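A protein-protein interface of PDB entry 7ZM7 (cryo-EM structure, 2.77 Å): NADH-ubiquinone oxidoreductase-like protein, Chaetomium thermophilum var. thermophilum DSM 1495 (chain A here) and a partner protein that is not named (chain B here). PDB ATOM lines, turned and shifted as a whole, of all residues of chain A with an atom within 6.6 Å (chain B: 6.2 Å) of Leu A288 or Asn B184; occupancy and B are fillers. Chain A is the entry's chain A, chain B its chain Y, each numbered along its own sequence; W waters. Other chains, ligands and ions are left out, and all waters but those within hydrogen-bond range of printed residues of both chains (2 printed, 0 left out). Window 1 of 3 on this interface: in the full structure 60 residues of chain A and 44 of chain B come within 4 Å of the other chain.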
ATOM      1  N   LYS A  77     -18.682  -6.434 -12.324  1.00  0.00           N
ATOM      2  CA  LYS A  77     -19.230  -5.563 -13.388  1.00  0.00           C
ATOM      3  C   LYS A  77     -20.724  -5.315 -13.200  1.00  0.00           C
ATOM      4  O   LYS A  77     -21.330  -4.778 -14.128  1.00  0.00           O
ATOM      5  CB  LYS A  77     -18.901  -6.210 -14.730  1.00  0.00           C
ATOM      6  CG  LYS A  77     -17.442  -6.560 -14.974  1.00  0.00           C
ATOM      7  CD  LYS A  77     -16.558  -5.347 -15.134  1.00  0.00           C
ATOM      8  CE  LYS A  77     -15.111  -5.699 -15.400  1.00  0.00           C
ATOM      9  NZ  LYS A  77     -14.234  -4.510 -15.314  1.00  0.00           N
ATOM     10  N   GLU A 260      -7.596 -19.743 -25.683  1.00  0.00           N
ATOM     11  CA  GLU A 260      -7.929 -18.297 -25.623  1.00  0.00           C
ATOM     12  C   GLU A 260      -7.797 -17.716 -27.027  1.00  0.00           C
ATOM     13  O   GLU A 260      -6.662 -17.596 -27.497  1.00  0.00           O
ATOM     14  CB  GLU A 260      -7.039 -17.594 -24.600  1.00  0.00           C
ATOM     15  CG  GLU A 260      -7.187 -18.172 -23.205  1.00  0.00           C
ATOM     16  CD  GLU A 260      -6.451 -17.435 -22.103  1.00  0.00           C
ATOM     17  OE1 GLU A 260      -6.422 -16.192 -22.138  1.00  0.00           O
ATOM     18  OE2 GLU A 260      -5.910 -18.109 -21.211  1.00  0.00           O
ATOM     19  N   ASN A 271     -12.511 -10.997 -27.076  1.00  0.00           N
ATOM     20  CA  ASN A 271     -11.673 -12.061 -26.557  1.00  0.00           C
ATOM     21  C   ASN A 271     -12.525 -13.156 -25.944  1.00  0.00           C
ATOM     22  O   ASN A 271     -13.398 -12.885 -25.121  1.00  0.00           O
ATOM     23  CB  ASN A 271     -10.704 -11.492 -25.528  1.00  0.00           C
ATOM     24  CG  ASN A 271      -9.659 -10.631 -26.157  1.00  0.00           C
ATOM     25  OD1 ASN A 271      -9.775  -9.426 -26.200  1.00  0.00           O
ATOM     26  ND2 ASN A 271      -8.634 -11.253 -26.667  1.00  0.00           N
ATOM     27  N   PRO A 286     -17.013 -16.035 -22.900  1.00  0.00           N
ATOM     28  CA  PRO A 286     -16.261 -14.774 -22.899  1.00  0.00           C
ATOM     29  C   PRO A 286     -15.038 -14.730 -21.962  1.00  0.00           C
ATOM     30  O   PRO A 286     -15.145 -15.214 -20.869  1.00  0.00           O
ATOM     31  CB  PRO A 286     -17.341 -13.776 -22.475  1.00  0.00           C
ATOM     32  CG  PRO A 286     -18.263 -14.553 -21.575  1.00  0.00           C
ATOM     33  CD  PRO A 286     -18.214 -15.979 -22.077  1.00  0.00           C
ATOM     34  N   ARG A 287     -13.897 -14.200 -22.408  1.00  0.00           N
ATOM     35  CA  ARG A 287     -12.735 -14.000 -21.496  1.00  0.00           C
ATOM     36  C   ARG A 287     -12.545 -12.493 -21.262  1.00  0.00           C
ATOM     37  O   ARG A 287     -12.945 -11.722 -22.144  1.00  0.00           O
ATOM     38  CB  ARG A 287     -11.485 -14.749 -21.970  1.00  0.00           C
ATOM     39  CG  ARG A 287     -10.730 -14.113 -23.123  1.00  0.00           C
ATOM     40  CD  ARG A 287      -9.540 -14.989 -23.430  1.00  0.00           C
ATOM     41  NE  ARG A 287      -8.992 -14.782 -24.759  1.00  0.00           N
ATOM     42  CZ  ARG A 287      -7.867 -14.133 -25.010  1.00  0.00           C
ATOM     43  NH1 ARG A 287      -7.166 -13.625 -24.013  1.00  0.00           N
ATOM     44  NH2 ARG A 287      -7.437 -14.009 -26.251  1.00  0.00           N
ATOM     45  N   LEU A 288     -11.975 -12.087 -20.123  1.00  0.00           N
ATOM     46  CA  LEU A 288     -11.850 -10.673 -19.810  1.00  0.00           C
ATOM     47  C   LEU A 288     -10.888  -9.957 -20.744  1.00  0.00           C
ATOM     48  O   LEU A 288      -9.787 -10.436 -21.020  1.00  0.00           O
ATOM     49  CB  LEU A 288     -11.418 -10.492 -18.360  1.00  0.00           C
ATOM     50  CG  LEU A 288     -11.400  -9.071 -17.814  1.00  0.00           C
ATOM     51  CD1 LEU A 288     -11.617  -9.127 -16.363  1.00  0.00           C
ATOM     52  CD2 LEU A 288     -10.051  -8.474 -18.019  1.00  0.00           C
ATOM     53  N   ASN A 289     -11.325  -8.793 -21.215  1.00  0.00           N
ATOM     54  CA  ASN A 289     -10.454  -7.818 -21.855  1.00  0.00           C
ATOM     55  C   ASN A 289     -11.159  -6.476 -21.696  1.00  0.00           C
ATOM     56  O   ASN A 289     -12.083  -6.175 -22.456  1.00  0.00           O
ATOM     57  CB  ASN A 289     -10.224  -8.151 -23.314  1.00  0.00           C
ATOM     58  CG  ASN A 289      -8.975  -7.537 -23.856  1.00  0.00           C
ATOM     59  OD1 ASN A 289      -8.705  -6.374 -23.634  1.00  0.00           O
ATOM     60  ND2 ASN A 289      -8.194  -8.320 -24.554  1.00  0.00           N
ATOM     61  N   ASP A 290     -10.722  -5.684 -20.722  1.00  0.00           N
ATOM     62  CA  ASP A 290     -11.407  -4.429 -20.453  1.00  0.00           C
ATOM     63  C   ASP A 290     -11.225  -3.412 -21.572  1.00  0.00           C
ATOM     64  O   ASP A 290     -11.994  -2.457 -21.654  1.00  0.00           O
ATOM     65  CB  ASP A 290     -10.938  -3.854 -19.127  1.00  0.00           C
ATOM     66  CG  ASP A 290     -11.815  -4.276 -17.970  1.00  0.00           C
ATOM     67  OD1 ASP A 290     -13.053  -4.214 -18.109  1.00  0.00           O
ATOM     68  OD2 ASP A 290     -11.272  -4.661 -16.916  1.00  0.00           O
ATOM     69  N   ASP A 291     -10.236  -3.608 -22.432  1.00  0.00           N
ATOM     70  CA  ASP A 291     -10.007  -2.734 -23.566  1.00  0.00           C
ATOM     71  C   ASP A 291     -10.955  -3.002 -24.713  1.00  0.00           C
ATOM     72  O   ASP A 291     -11.099  -2.142 -25.584  1.00  0.00           O
ATOM     73  CB  ASP A 291      -8.575  -2.901 -24.056  1.00  0.00           C
ATOM     74  CG  ASP A 291      -7.583  -2.792 -22.940  1.00  0.00           C
ATOM     75  OD1 ASP A 291      -7.631  -1.781 -22.210  1.00  0.00           O
ATOM     76  OD2 ASP A 291      -6.768  -3.721 -22.768  1.00  0.00           O
ATOM     77  N   ASN A 293     -14.071  -5.955 -24.744  1.00  0.00           N
ATOM     78  CA  ASN A 293     -15.400  -6.540 -24.592  1.00  0.00           C
ATOM     79  C   ASN A 293     -15.876  -6.717 -23.158  1.00  0.00           C
ATOM     80  O   ASN A 293     -17.084  -6.828 -22.950  1.00  0.00           O
ATOM     81  CB  ASN A 293     -15.484  -7.902 -25.297  1.00  0.00           C
ATOM     82  CG  ASN A 293     -14.436  -8.878 -24.829  1.00  0.00           C
ATOM     83  OD1 ASN A 293     -13.250  -8.615 -24.917  1.00  0.00           O
ATOM     84  ND2 ASN A 293     -14.875 -10.022 -24.348  1.00  0.00           N
ATOM     85  N   GLU A 294     -14.953  -6.678 -22.189  1.00  0.00           N
ATOM     86  CA  GLU A 294     -15.279  -6.618 -20.736  1.00  0.00           C
ATOM     87  C   GLU A 294     -16.184  -7.740 -20.189  1.00  0.00           C
ATOM     88  O   GLU A 294     -17.205  -7.424 -19.553  1.00  0.00           O
ATOM     89  CB  GLU A 294     -15.930  -5.241 -20.567  1.00  0.00           C
ATOM     90  CG  GLU A 294     -15.991  -4.697 -19.160  1.00  0.00           C
ATOM     91  CD  GLU A 294     -16.883  -3.476 -19.039  1.00  0.00           C
ATOM     92  OE1 GLU A 294     -17.267  -2.926 -20.091  1.00  0.00           O
ATOM     93  OE2 GLU A 294     -17.194  -3.082 -17.899  1.00  0.00           O
ATOM     94  N   GLU A 295     -15.794  -9.006 -20.346  1.00  0.00           N
ATOM     95  CA  GLU A 295     -16.559 -10.117 -19.713  1.00  0.00           C
ATOM     96  C   GLU A 295     -17.858 -10.390 -20.455  1.00  0.00           C
ATOM     97  O   GLU A 295     -18.630 -11.223 -19.972  1.00  0.00           O
ATOM     98  CB  GLU A 295     -16.957  -9.790 -18.273  1.00  0.00           C
ATOM     99  CG  GLU A 295     -15.801  -9.831 -17.291  1.00  0.00           C
ATOM    100  CD  GLU A 295     -15.893 -10.949 -16.269  1.00  0.00           C
ATOM    101  OE1 GLU A 295     -16.716 -11.861 -16.471  1.00  0.00           O
ATOM    102  OE2 GLU A 295     -15.151 -10.899 -15.269  1.00  0.00           O
ATOM    103  N   TRP A 296     -18.070  -9.749 -21.591  1.00  0.00           N
ATOM    104  CA  TRP A 296     -19.364  -9.898 -22.286  1.00  0.00           C
ATOM    105  C   TRP A 296     -19.112 -10.281 -23.731  1.00  0.00           C
ATOM    106  O   TRP A 296     -18.101  -9.824 -24.275  1.00  0.00           O
ATOM    107  CB  TRP A 296     -20.186  -8.603 -22.254  1.00  0.00           C
ATOM    108  CG  TRP A 296     -20.278  -7.855 -20.959  1.00  0.00           C
ATOM    109  CD1 TRP A 296     -20.007  -6.530 -20.773  1.00  0.00           C
ATOM    110  CD2 TRP A 296     -20.715  -8.354 -19.682  1.00  0.00           C
ATOM    111  NE1 TRP A 296     -20.221  -6.177 -19.470  1.00  0.00           N
ATOM    112  CE2 TRP A 296     -20.654  -7.274 -18.776  1.00  0.00           C
ATOM    113  CE3 TRP A 296     -21.138  -9.602 -19.211  1.00  0.00           C
ATOM    114  CZ2 TRP A 296     -20.999  -7.409 -17.434  1.00  0.00           C
ATOM    115  CZ3 TRP A 296     -21.469  -9.736 -17.882  1.00  0.00           C
ATOM    116  CH2 TRP A 296     -21.404  -8.651 -17.009  1.00  0.00           C
ATOM    117  N   ARG A 611      -6.266  -2.693 -32.844  1.00  0.00           N
ATOM    118  CA  ARG A 611      -5.526  -3.632 -32.022  1.00  0.00           C
ATOM    119  C   ARG A 611      -5.312  -4.912 -32.813  1.00  0.00           C
ATOM    120  O   ARG A 611      -6.257  -5.473 -33.372  1.00  0.00           O
ATOM    121  CB  ARG A 611      -6.267  -3.902 -30.718  1.00  0.00           C
ATOM    122  CG  ARG A 611      -5.605  -4.874 -29.804  1.00  0.00           C
ATOM    123  CD  ARG A 611      -6.382  -4.998 -28.517  1.00  0.00           C
ATOM    124  NE  ARG A 611      -6.935  -3.723 -28.091  1.00  0.00           N
ATOM    125  CZ  ARG A 611      -6.414  -2.971 -27.131  1.00  0.00           C
ATOM    126  NH1 ARG A 611      -5.340  -3.375 -26.480  1.00  0.00           N
ATOM    127  NH2 ARG A 611      -6.981  -1.819 -26.817  1.00  0.00           N
ATOM    128  N   GLN A 613      -4.669  -8.627 -32.913  1.00  0.00           N
ATOM    129  CA  GLN A 613      -4.799  -9.813 -32.036  1.00  0.00           C
ATOM    130  C   GLN A 613      -4.564 -11.088 -32.846  1.00  0.00           C
ATOM    131  O   GLN A 613      -4.645 -11.018 -34.070  1.00  0.00           O
ATOM    132  CB  GLN A 613      -6.133  -9.735 -31.298  1.00  0.00           C
ATOM    133  CG  GLN A 613      -6.308  -8.467 -30.477  1.00  0.00           C
ATOM    134  CD  GLN A 613      -7.633  -8.430 -29.761  1.00  0.00           C
ATOM    135  OE1 GLN A 613      -7.701  -8.534 -28.540  1.00  0.00           O
ATOM    136  NE2 GLN A 613      -8.705  -8.277 -30.517  1.00  0.00           N
ATOM    137  N   ASP A 666      -1.705  -7.565 -29.367  1.00  0.00           N
ATOM    138  CA  ASP A 666      -2.574  -7.226 -28.245  1.00  0.00           C
ATOM    139  C   ASP A 666      -2.412  -5.782 -27.817  1.00  0.00           C
ATOM    140  O   ASP A 666      -2.675  -5.433 -26.668  1.00  0.00           O
ATOM    141  CB  ASP A 666      -2.350  -8.149 -27.039  1.00  0.00           C
ATOM    142  CG  ASP A 666      -2.386  -9.617 -27.403  1.00  0.00           C
ATOM    143  OD1 ASP A 666      -3.042  -9.969 -28.403  1.00  0.00           O
ATOM    144  OD2 ASP A 666      -1.770 -10.417 -26.670  1.00  0.00           O
ATOM    145  N   ALA B 113      -6.885 -17.433 -18.345  1.00  0.00           N
ATOM    146  CA  ALA B 113      -7.914 -16.487 -17.963  1.00  0.00           C
ATOM    147  C   ALA B 113      -8.883 -17.140 -16.999  1.00  0.00           C
ATOM    148  O   ALA B 113      -9.082 -18.355 -17.016  1.00  0.00           O
ATOM    149  CB  ALA B 113      -8.661 -15.979 -19.191  1.00  0.00           C
ATOM    150  N   LYS B 114      -9.475 -16.327 -16.145  1.00  0.00           N
ATOM    151  CA  LYS B 114     -10.477 -16.841 -15.236  1.00  0.00           C
ATOM    152  C   LYS B 114     -11.677 -17.346 -16.032  1.00  0.00           C
ATOM    153  O   LYS B 114     -12.043 -16.746 -17.046  1.00  0.00           O
ATOM    154  CB  LYS B 114     -10.902 -15.759 -14.250  1.00  0.00           C
ATOM    155  CG  LYS B 114     -11.967 -16.209 -13.279  1.00  0.00           C
ATOM    156  CD  LYS B 114     -12.561 -15.060 -12.515  1.00  0.00           C
ATOM    157  CE  LYS B 114     -13.315 -14.160 -13.427  1.00  0.00           C
ATOM    158  NZ  LYS B 114     -14.433 -14.878 -14.105  1.00  0.00           N
ATOM    159  N   GLN B 181       1.778 -14.568 -24.465  1.00  0.00           N
ATOM    160  CA  GLN B 181       0.557 -13.733 -24.470  1.00  0.00           C
ATOM    161  C   GLN B 181       0.517 -12.955 -23.152  1.00  0.00           C
ATOM    162  O   GLN B 181       0.511 -13.596 -22.095  1.00  0.00           O
ATOM    163  CB  GLN B 181      -0.665 -14.603 -24.765  1.00  0.00           C
ATOM    164  CG  GLN B 181      -1.990 -14.018 -24.307  1.00  0.00           C
ATOM    165  CD  GLN B 181      -3.044 -15.094 -24.229  1.00  0.00           C
ATOM    166  OE1 GLN B 181      -4.054 -14.957 -23.544  1.00  0.00           O
ATOM    167  NE2 GLN B 181      -2.803 -16.194 -24.922  1.00  0.00           N
ATOM    168  N   GLU B 182       0.510 -11.624 -23.223  1.00  0.00           N
ATOM    169  CA  GLU B 182       0.545 -10.780 -21.996  1.00  0.00           C
ATOM    170  C   GLU B 182      -0.810 -10.843 -21.272  1.00  0.00           C
ATOM    171  O   GLU B 182      -1.826 -10.725 -21.970  1.00  0.00           O
ATOM    172  CB  GLU B 182       0.954  -9.347 -22.337  1.00  0.00           C
ATOM    173  CG  GLU B 182       0.920  -8.394 -21.155  1.00  0.00           C
ATOM    174  CD  GLU B 182       1.868  -8.719 -20.012  1.00  0.00           C
ATOM    175  OE1 GLU B 182       2.907  -9.364 -20.267  1.00  0.00           O
ATOM    176  OE2 GLU B 182       1.553  -8.343 -18.863  1.00  0.00           O
ATOM    177  N   PRO B 183      -0.905 -11.072 -19.938  1.00  0.00           N
ATOM    178  CA  PRO B 183      -2.214 -11.169 -19.298  1.00  0.00           C
ATOM    179  C   PRO B 183      -3.087  -9.953 -19.559  1.00  0.00           C
ATOM    180  O   PRO B 183      -2.605  -8.832 -19.713  1.00  0.00           O
ATOM    181  CB  PRO B 183      -1.861 -11.282 -17.816  1.00  0.00           C
ATOM    182  CG  PRO B 183      -0.545 -11.875 -17.796  1.00  0.00           C
ATOM    183  CD  PRO B 183       0.169 -11.499 -19.036  1.00  0.00           C
ATOM    184  N   ASN B 184      -4.386 -10.191 -19.612  1.00  0.00           N
ATOM    185  CA  ASN B 184      -5.387  -9.138 -19.570  1.00  0.00           C
ATOM    186  C   ASN B 184      -5.787  -8.923 -18.118  1.00  0.00           C
ATOM    187  O   ASN B 184      -6.215  -9.868 -17.448  1.00  0.00           O
ATOM    188  CB  ASN B 184      -6.610  -9.513 -20.398  1.00  0.00           C
ATOM    189  CG  ASN B 184      -6.442  -9.204 -21.845  1.00  0.00           C
ATOM    190  OD1 ASN B 184      -6.777 -10.015 -22.705  1.00  0.00           O
ATOM    191  ND2 ASN B 184      -5.902  -8.031 -22.136  1.00  0.00           N
ATOM    192  N   GLU B 185      -5.649  -7.701 -17.630  1.00  0.00           N
ATOM    193  CA  GLU B 185      -5.982  -7.386 -16.251  1.00  0.00           C
ATOM    194  C   GLU B 185      -7.187  -6.460 -16.193  1.00  0.00           C
ATOM    195  O   GLU B 185      -7.583  -5.851 -17.183  1.00  0.00           O
ATOM    196  CB  GLU B 185      -4.794  -6.739 -15.539  1.00  0.00           C
ATOM    197  CG  GLU B 185      -3.603  -7.657 -15.403  1.00  0.00           C
ATOM    198  CD  GLU B 185      -3.881  -8.837 -14.497  1.00  0.00           C
ATOM    199  OE1 GLU B 185      -4.657  -8.678 -13.532  1.00  0.00           O
ATOM    200  OE2 GLU B 185      -3.330  -9.926 -14.757  1.00  0.00           O
ATOM    201  N   ARG B 186      -7.766  -6.353 -15.012  1.00  0.00           N
ATOM    202  CA  ARG B 186      -8.906  -5.480 -14.852  1.00  0.00           C
ATOM    203  C   ARG B 186      -8.468  -4.030 -14.739  1.00  0.00           C
ATOM    204  O   ARG B 186      -7.292  -3.716 -14.559  1.00  0.00           O
ATOM    205  CB  ARG B 186      -9.712  -5.849 -13.609  1.00  0.00           C
ATOM    206  CG  ARG B 186     -10.542  -7.072 -13.746  1.00  0.00           C
ATOM    207  CD  ARG B 186     -11.662  -7.060 -12.744  1.00  0.00           C
ATOM    208  NE  ARG B 186     -12.076  -8.412 -12.387  1.00  0.00           N
ATOM    209  CZ  ARG B 186     -13.069  -9.073 -12.968  1.00  0.00           C
ATOM    210  NH1 ARG B 186     -13.769  -8.516 -13.946  1.00  0.00           N
ATOM    211  NH2 ARG B 186     -13.362 -10.295 -12.562  1.00  0.00           N
HETATM  212  O   HOH W   1      -5.877 -10.497 -25.504  1.00  0.00           O
HETATM  213  O   HOH W   2     -11.992 -14.204 -17.601  1.00  0.00           O
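O of Leu A288 sits close to OD1 of Asn B184, at 3.5 Å. The side-chain carboxylate (OE1) of Glu A260 lies close to the side-chain amide oxygen (OE1) of Gln B181 (3.0 Å). The side-chain amide oxygen (OD1) of Asn B184 is in hydrogen-bond range of the side-chain amide nitrogen (ND2) of Asn A289 (2.9 Å). The backbone NH (N) of Ala B113 is in hydrogen-bond range of the side-chain carboxylate (OE2) of Glu A260 (3.1 Å). OE1 of Gln B181 is in hydrogen-bond range of NH1 of Arg A287, at 3.4 Å. NH1 of Arg B186 is in salt-bridge range of OE2 of Glu A295.
O of Arg A287 lies within hydrogen-bond range of ND2 of Asn A293, 3.4 Å away. The backbone NH (N) of Glu A294 sits at hydrogen-bond distance from the backbone carbonyl oxygen (O) of Asn A289. The side-chain amino group of Lys A77 lies within salt-bridge range of the side-chain carboxylate of Asp A290, 3.0 Å away. The backbone NH (N) of Asp A291 sits close to the side-chain amide oxygen (OD1) of Asn A289, 3.4 Å away. The guanidinium group (NH1) of Arg A287 lies within salt-bridge range of the side-chain carboxylate (OE1) of Glu A260 (3.3 Å). OD1 of Asn A271 lies within hydrogen-bond range of ND2 of Asn A289 (2.5 Å).
CE of Lys A77 touches NH1 of Arg B186, at 3.4 Å. Asn B184 touches Arg A287 (OD1 to NH1, 3.9 Å). Glu B185 touches Leu A288 (O to CD2, 3.7 Å). Arg B186 touches Leu A288 (NH1 to CD1, 3.3 Å). Asp A290 touches Glu B185 (OD2 to O, 3.9 Å). Asp A290 touches Arg B186 (OD2 to CA, 3.2 Å).
Printed residues of chain B within 4 Å of Lys A77: Arg B186 (3.4 Å). Leu A288 touches just these residues of chain B: Asn B184, Glu B185 and Arg B186. Of the printed residues of chain B, Asn A289 touches Asn B184. Printed residues of chain B within 4 Å of Glu A295: Arg B186. Of the printed residues of chain A, Gln B181 touches Glu A260 (3.0 Å) and Arg A287 (3.4 Å). Of the printed residues of chain A, Glu B185 touches Leu A288 and Asp A290. The nearest residue of chain A that does not touch Asn B184 is Asp A291 (4.4 Å).
Printed residues of chain A that touch a printed residue of chain B: Lys A77, Glu A260, Arg A287, Leu A288, Asn A289, Asp A290 and Glu A295. Of the 8 printed residues of chain B, 5 touch a printed residue of chain A. Printed residues of chain B that touch a printed residue of chain A: Ala B113, Gln B181, Asn B184, Glu B185 and Arg B186. Hydrophobic or aromatic side chains of chain B within 4 Å of the printed part of chain A: Ala B113. Among the printed residues, Asp or Glu carboxylates within 4 Å of a Lys or Arg side-chain nitrogen of the other chain: Glu A295 with Arg B186 (3.1 Å).
Water W2 lies within hydrogen-bond range of O of Lys B114 (2.6 Å) and N of Leu A288 (3.3 Å). Water W1 lies within hydrogen-bond range of OD1 of Asn B184 (3.0 Å), ND2 of Asn A271 (3.1 Å) and ND2 of Asn A289 (3.3 Å).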
